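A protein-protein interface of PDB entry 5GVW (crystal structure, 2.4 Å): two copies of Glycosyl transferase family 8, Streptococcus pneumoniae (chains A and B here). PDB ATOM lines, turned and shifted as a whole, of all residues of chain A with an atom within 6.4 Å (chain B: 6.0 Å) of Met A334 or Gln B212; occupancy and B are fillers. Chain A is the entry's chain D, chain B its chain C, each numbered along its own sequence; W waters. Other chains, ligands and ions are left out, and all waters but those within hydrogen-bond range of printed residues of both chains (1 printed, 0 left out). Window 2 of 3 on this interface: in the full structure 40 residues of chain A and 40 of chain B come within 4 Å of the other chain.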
ATOM      1  N   TYR A 309      23.231   1.685 -13.518  1.00  0.00           N
ATOM      2  CA  TYR A 309      22.474   0.449 -13.630  1.00  0.00           C
ATOM      3  C   TYR A 309      22.424  -0.333 -12.311  1.00  0.00           C
ATOM      4  O   TYR A 309      21.860  -1.419 -12.261  1.00  0.00           O
ATOM      5  CB  TYR A 309      23.059  -0.417 -14.763  1.00  0.00           C
ATOM      6  CG  TYR A 309      22.953   0.153 -16.175  1.00  0.00           C
ATOM      7  CD1 TYR A 309      22.059   1.181 -16.487  1.00  0.00           C
ATOM      8  CD2 TYR A 309      23.718  -0.390 -17.232  1.00  0.00           C
ATOM      9  CE1 TYR A 309      21.956   1.675 -17.784  1.00  0.00           C
ATOM     10  CE2 TYR A 309      23.607   0.098 -18.533  1.00  0.00           C
ATOM     11  CZ  TYR A 309      22.721   1.136 -18.789  1.00  0.00           C
ATOM     12  OH  TYR A 309      22.580   1.670 -20.034  1.00  0.00           O
ATOM     13  N   LEU A 332      18.035   1.396 -16.439  1.00  0.00           N
ATOM     14  CA  LEU A 332      18.230   0.389 -17.470  1.00  0.00           C
ATOM     15  C   LEU A 332      18.541   1.046 -18.800  1.00  0.00           C
ATOM     16  O   LEU A 332      18.292   2.208 -18.958  1.00  0.00           O
ATOM     17  CB  LEU A 332      17.012  -0.512 -17.568  1.00  0.00           C
ATOM     18  CG  LEU A 332      16.807  -1.373 -16.334  1.00  0.00           C
ATOM     19  CD1 LEU A 332      15.369  -1.792 -16.166  1.00  0.00           C
ATOM     20  CD2 LEU A 332      17.712  -2.568 -16.372  1.00  0.00           C
ATOM     21  N   PRO A 333      19.095   0.298 -19.749  1.00  0.00           N
ATOM     22  CA  PRO A 333      19.496   0.842 -21.062  1.00  0.00           C
ATOM     23  C   PRO A 333      18.435   1.644 -21.819  1.00  0.00           C
ATOM     24  O   PRO A 333      18.721   2.744 -22.325  1.00  0.00           O
ATOM     25  CB  PRO A 333      19.930  -0.398 -21.835  1.00  0.00           C
ATOM     26  CG  PRO A 333      20.402  -1.376 -20.784  1.00  0.00           C
ATOM     27  CD  PRO A 333      19.695  -1.039 -19.499  1.00  0.00           C
ATOM     28  N   MET A 334      17.213   1.132 -21.863  1.00  0.00           N
ATOM     29  CA  MET A 334      16.144   1.807 -22.611  1.00  0.00           C
ATOM     30  C   MET A 334      15.705   3.096 -21.933  1.00  0.00           C
ATOM     31  O   MET A 334      15.151   3.987 -22.568  1.00  0.00           O
ATOM     32  CB  MET A 334      14.954   0.870 -22.846  1.00  0.00           C
ATOM     33  CG  MET A 334      15.178  -0.132 -23.973  1.00  0.00           C
ATOM     34  SD  MET A 334      13.918  -1.439 -24.111  1.00  0.00           S
ATOM     35  CE  MET A 334      14.822  -2.594 -25.160  1.00  0.00           C
ATOM     36  N   LEU A 335      15.952   3.202 -20.641  1.00  0.00           N
ATOM     37  CA  LEU A 335      15.581   4.406 -19.902  1.00  0.00           C
ATOM     38  C   LEU A 335      16.679   5.405 -20.058  1.00  0.00           C
ATOM     39  O   LEU A 335      16.408   6.572 -20.284  1.00  0.00           O
ATOM     40  CB  LEU A 335      15.347   4.076 -18.437  1.00  0.00           C
ATOM     41  CG  LEU A 335      14.265   3.012 -18.263  1.00  0.00           C
ATOM     42  CD1 LEU A 335      14.349   2.424 -16.868  1.00  0.00           C
ATOM     43  CD2 LEU A 335      12.885   3.594 -18.555  1.00  0.00           C
ATOM     44  N   LEU A 336      17.927   4.937 -19.942  1.00  0.00           N
ATOM     45  CA  LEU A 336      19.095   5.741 -20.356  1.00  0.00           C
ATOM     46  C   LEU A 336      18.905   6.314 -21.772  1.00  0.00           C
ATOM     47  O   LEU A 336      19.142   7.502 -22.013  1.00  0.00           O
ATOM     48  CB  LEU A 336      20.387   4.910 -20.290  1.00  0.00           C
ATOM     49  CG  LEU A 336      21.766   5.613 -20.249  1.00  0.00           C
ATOM     50  CD1 LEU A 336      22.592   5.324 -21.476  1.00  0.00           C
ATOM     51  CD2 LEU A 336      21.697   7.125 -20.078  1.00  0.00           C
ATOM     52  N   GLU A 337      18.449   5.468 -22.689  1.00  0.00           N
ATOM     53  CA  GLU A 337      18.257   5.853 -24.072  1.00  0.00           C
ATOM     54  C   GLU A 337      17.312   7.066 -24.223  1.00  0.00           C
ATOM     55  O   GLU A 337      17.622   8.012 -24.959  1.00  0.00           O
ATOM     56  CB  GLU A 337      17.776   4.631 -24.880  1.00  0.00           C
ATOM     57  CG  GLU A 337      17.474   4.912 -26.355  1.00  0.00           C
ATOM     58  CD  GLU A 337      17.108   3.660 -27.142  1.00  0.00           C
ATOM     59  OE1 GLU A 337      16.987   2.569 -26.545  1.00  0.00           O
ATOM     60  OE2 GLU A 337      16.947   3.776 -28.378  1.00  0.00           O
ATOM     61  N   GLN A 338      16.183   7.051 -23.505  1.00  0.00           N
ATOM     62  CA  GLN A 338      15.249   8.168 -23.567  1.00  0.00           C
ATOM     63  C   GLN A 338      15.875   9.449 -23.041  1.00  0.00           C
ATOM     64  O   GLN A 338      15.644  10.530 -23.589  1.00  0.00           O
ATOM     65  CB  GLN A 338      13.921   7.850 -22.854  1.00  0.00           C
ATOM     66  CG  GLN A 338      13.073   6.736 -23.488  1.00  0.00           C
ATOM     67  CD  GLN A 338      12.915   6.813 -25.020  1.00  0.00           C
ATOM     68  OE1 GLN A 338      12.501   7.838 -25.570  1.00  0.00           O
ATOM     69  NE2 GLN A 338      13.255   5.721 -25.710  1.00  0.00           N
ATOM     70  N   ILE A 339      16.700   9.330 -22.009  1.00  0.00           N
ATOM     71  CA  ILE A 339      17.406  10.487 -21.461  1.00  0.00           C
ATOM     72  C   ILE A 339      18.383  11.047 -22.489  1.00  0.00           C
ATOM     73  O   ILE A 339      18.411  12.266 -22.709  1.00  0.00           O
ATOM     74  CB  ILE A 339      18.109  10.165 -20.126  1.00  0.00           C
ATOM     75  CG1 ILE A 339      17.042   9.863 -19.075  1.00  0.00           C
ATOM     76  CG2 ILE A 339      18.942  11.346 -19.647  1.00  0.00           C
ATOM     77  CD1 ILE A 339      17.581   9.297 -17.777  1.00  0.00           C
ATOM     78  N   PHE A 361      24.281   5.035 -28.059  1.00  0.00           N
ATOM     79  CA  PHE A 361      23.181   6.007 -28.156  1.00  0.00           C
ATOM     80  C   PHE A 361      23.656   7.411 -28.558  1.00  0.00           C
ATOM     81  O   PHE A 361      22.951   8.121 -29.237  1.00  0.00           O
ATOM     82  CB  PHE A 361      22.353   6.114 -26.853  1.00  0.00           C
ATOM     83  CG  PHE A 361      21.861   4.799 -26.296  1.00  0.00           C
ATOM     84  CD1 PHE A 361      21.277   3.837 -27.108  1.00  0.00           C
ATOM     85  CD2 PHE A 361      21.961   4.540 -24.940  1.00  0.00           C
ATOM     86  CE1 PHE A 361      20.841   2.618 -26.584  1.00  0.00           C
ATOM     87  CE2 PHE A 361      21.525   3.335 -24.403  1.00  0.00           C
ATOM     88  CZ  PHE A 361      20.957   2.371 -25.226  1.00  0.00           C
ATOM     89  N   ALA B 206       9.094  -2.567 -18.734  1.00  0.00           N
ATOM     90  CA  ALA B 206       9.295  -2.549 -20.182  1.00  0.00           C
ATOM     91  C   ALA B 206      10.754  -2.449 -20.576  1.00  0.00           C
ATOM     92  O   ALA B 206      11.124  -2.953 -21.620  1.00  0.00           O
ATOM     93  CB  ALA B 206       8.520  -1.405 -20.814  1.00  0.00           C
ATOM     94  N   ALA B 207      11.561  -1.759 -19.769  1.00  0.00           N
ATOM     95  CA  ALA B 207      13.021  -1.760 -19.954  1.00  0.00           C
ATOM     96  C   ALA B 207      13.644  -3.093 -19.546  1.00  0.00           C
ATOM     97  O   ALA B 207      14.597  -3.510 -20.153  1.00  0.00           O
ATOM     98  CB  ALA B 207      13.677  -0.612 -19.191  1.00  0.00           C
ATOM     99  N   PHE B 209      12.299  -6.239 -19.571  1.00  0.00           N
ATOM    100  CA  PHE B 209      11.970  -7.309 -20.510  1.00  0.00           C
ATOM    101  C   PHE B 209      12.234  -6.891 -21.957  1.00  0.00           C
ATOM    102  O   PHE B 209      11.880  -7.599 -22.878  1.00  0.00           O
ATOM    103  CB  PHE B 209      10.507  -7.765 -20.313  1.00  0.00           C
ATOM    104  CG  PHE B 209      10.232  -8.390 -18.954  1.00  0.00           C
ATOM    105  CD1 PHE B 209      10.822  -9.612 -18.593  1.00  0.00           C
ATOM    106  CD2 PHE B 209       9.370  -7.770 -18.040  1.00  0.00           C
ATOM    107  CE1 PHE B 209      10.565 -10.192 -17.351  1.00  0.00           C
ATOM    108  CE2 PHE B 209       9.111  -8.351 -16.796  1.00  0.00           C
ATOM    109  CZ  PHE B 209       9.713  -9.562 -16.451  1.00  0.00           C
ATOM    110  N   LYS B 210      12.866  -5.741 -22.145  1.00  0.00           N
ATOM    111  CA  LYS B 210      13.321  -5.274 -23.458  1.00  0.00           C
ATOM    112  C   LYS B 210      12.185  -5.095 -24.490  1.00  0.00           C
ATOM    113  O   LYS B 210      12.373  -5.321 -25.689  1.00  0.00           O
ATOM    114  CB  LYS B 210      14.493  -6.141 -23.975  1.00  0.00           C
ATOM    115  CG  LYS B 210      15.833  -5.755 -23.359  1.00  0.00           C
ATOM    116  CD  LYS B 210      16.884  -6.845 -23.499  1.00  0.00           C
ATOM    117  CE  LYS B 210      16.751  -7.899 -22.413  1.00  0.00           C
ATOM    118  NZ  LYS B 210      17.961  -8.762 -22.371  1.00  0.00           N
ATOM    119  N   HIS B 211      11.025  -4.654 -24.009  1.00  0.00           N
ATOM    120  CA  HIS B 211       9.932  -4.229 -24.866  1.00  0.00           C
ATOM    121  C   HIS B 211      10.214  -2.836 -25.441  1.00  0.00           C
ATOM    122  O   HIS B 211       9.615  -1.839 -25.019  1.00  0.00           O
ATOM    123  CB  HIS B 211       8.613  -4.253 -24.098  1.00  0.00           C
ATOM    124  CG  HIS B 211       8.243  -5.611 -23.588  1.00  0.00           C
ATOM    125  ND1 HIS B 211       7.544  -5.808 -22.416  1.00  0.00           N
ATOM    126  CD2 HIS B 211       8.486  -6.845 -24.084  1.00  0.00           C
ATOM    127  CE1 HIS B 211       7.369  -7.103 -22.213  1.00  0.00           C
ATOM    128  NE2 HIS B 211       7.924  -7.753 -23.215  1.00  0.00           N
ATOM    129  N   GLN B 212      11.095  -2.786 -26.446  1.00  0.00           N
ATOM    130  CA  GLN B 212      11.573  -1.498 -27.010  1.00  0.00           C
ATOM    131  C   GLN B 212      10.486  -0.613 -27.595  1.00  0.00           C
ATOM    132  O   GLN B 212      10.621   0.604 -27.600  1.00  0.00           O
ATOM    133  CB  GLN B 212      12.702  -1.697 -28.053  1.00  0.00           C
ATOM    134  CG  GLN B 212      12.318  -2.443 -29.334  1.00  0.00           C
ATOM    135  CD  GLN B 212      13.506  -2.989 -30.126  1.00  0.00           C
ATOM    136  OE1 GLN B 212      14.671  -2.622 -29.891  1.00  0.00           O
ATOM    137  NE2 GLN B 212      13.214  -3.876 -31.074  1.00  0.00           N
ATOM    138  N   PHE B 213       9.404  -1.220 -28.078  1.00  0.00           N
ATOM    139  CA  PHE B 213       8.392  -0.481 -28.830  1.00  0.00           C
ATOM    140  C   PHE B 213       7.460   0.266 -27.896  1.00  0.00           C
ATOM    141  O   PHE B 213       6.893   1.301 -28.260  1.00  0.00           O
ATOM    142  CB  PHE B 213       7.629  -1.410 -29.785  1.00  0.00           C
ATOM    143  CG  PHE B 213       8.501  -2.047 -30.833  1.00  0.00           C
ATOM    144  CD1 PHE B 213       8.978  -1.296 -31.904  1.00  0.00           C
ATOM    145  CD2 PHE B 213       8.848  -3.394 -30.749  1.00  0.00           C
ATOM    146  CE1 PHE B 213       9.781  -1.870 -32.873  1.00  0.00           C
ATOM    147  CE2 PHE B 213       9.649  -3.984 -31.716  1.00  0.00           C
ATOM    148  CZ  PHE B 213      10.126  -3.215 -32.775  1.00  0.00           C
ATOM    149  N   ILE B 214       7.352  -0.222 -26.670  1.00  0.00           N
ATOM    150  CA  ILE B 214       6.728   0.568 -25.612  1.00  0.00           C
ATOM    151  C   ILE B 214       7.186   2.044 -25.661  1.00  0.00           C
ATOM    152  O   ILE B 214       6.390   2.949 -25.500  1.00  0.00           O
ATOM    153  CB  ILE B 214       7.050  -0.006 -24.209  1.00  0.00           C
ATOM    154  CG1 ILE B 214       6.411  -1.384 -23.995  1.00  0.00           C
ATOM    155  CG2 ILE B 214       6.614   0.958 -23.109  1.00  0.00           C
ATOM    156  CD1 ILE B 214       4.907  -1.393 -24.022  1.00  0.00           C
ATOM    157  N   PHE B 215       8.479   2.247 -25.885  1.00  0.00           N
ATOM    158  CA  PHE B 215       9.117   3.568 -25.810  1.00  0.00           C
ATOM    159  C   PHE B 215       8.889   4.486 -27.015  1.00  0.00           C
ATOM    160  O   PHE B 215       9.242   5.665 -26.961  1.00  0.00           O
ATOM    161  CB  PHE B 215      10.605   3.396 -25.501  1.00  0.00           C
ATOM    162  CG  PHE B 215      10.839   2.770 -24.167  1.00  0.00           C
ATOM    163  CD1 PHE B 215      10.799   3.533 -23.019  1.00  0.00           C
ATOM    164  CD2 PHE B 215      11.020   1.404 -24.048  1.00  0.00           C
ATOM    165  CE1 PHE B 215      10.970   2.952 -21.772  1.00  0.00           C
ATOM    166  CE2 PHE B 215      11.193   0.805 -22.797  1.00  0.00           C
ATOM    167  CZ  PHE B 215      11.171   1.583 -21.657  1.00  0.00           C
ATOM    168  N   ASP B 216       8.291   3.949 -28.079  1.00  0.00           N
ATOM    169  CA  ASP B 216       7.913   4.754 -29.235  1.00  0.00           C
ATOM    170  C   ASP B 216       6.504   5.301 -29.107  1.00  0.00           C
ATOM    171  O   ASP B 216       6.110   6.148 -29.928  1.00  0.00           O
ATOM    172  CB  ASP B 216       8.085   3.966 -30.554  1.00  0.00           C
ATOM    173  CG  ASP B 216       9.540   3.554 -30.819  1.00  0.00           C
ATOM    174  OD1 ASP B 216       9.738   2.481 -31.438  1.00  0.00           O
ATOM    175  OD2 ASP B 216      10.483   4.288 -30.398  1.00  0.00           O
HETATM  176  O   HOH W   1      16.832  -1.564 -21.629  1.00  0.00           O
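Among the printed residues, pairs that only touch across the chains: Met A334 with Lys B210 (3.5 Å), Gln A338 with Phe B215 (3.5 Å), Leu A332 with Ala B207 (3.7 Å), Met A334 with Gln B212 (3.7 Å), Met A334 with Phe B215 (3.8 Å), Leu A335 with Ala B207 (3.8 Å) and Leu A335 with Phe B215 (3.8 Å).
Printed residues of chain B that touch a printed residue of chain A: Ala B207, Lys B210, Gln B212 and Phe B215. Hydrophobic or aromatic side chains of chain B within 4 Å of the printed part of chain A: Ala B207 and Phe B215. Of the 10 printed residues of chain A, 4 touch a printed residue of chain B. Among the printed residues, 7 pairs touch across the chains.
Tyr A309 touches none of the printed residues of chain B. Of the printed residues of chain B, Leu A332 touches Ala B207. Of chain B, only Lys B210 (3.5 Å), Gln B212 (3.7 Å) and Phe B215 (3.8 Å) come within 4 Å of Met A334. Printed residues of chain B within 4 Å of Leu A335: Ala B207 and Phe B215. Printed residues of chain A within 4 Å of Ala B207: Leu A332 and Leu A335. Printed residues of chain A within 4 Å of Lys B210: Met A334 (3.5 Å). Of the printed residues of chain A, Phe B215 touches Met A334 (3.8 Å), Leu A335 (3.8 Å) and Gln A338 (3.5 Å). The nearest printed residue of chain B that does not touch Leu A332 is Phe B209 (6.4 Å).
Water W1 lies within hydrogen-bond range of the backbone NH (N) of Met A334 (2.7 Å) and the backbone carbonyl oxygen (O) of Ala B207 (3.3 Å).
No position is printed for both chains.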
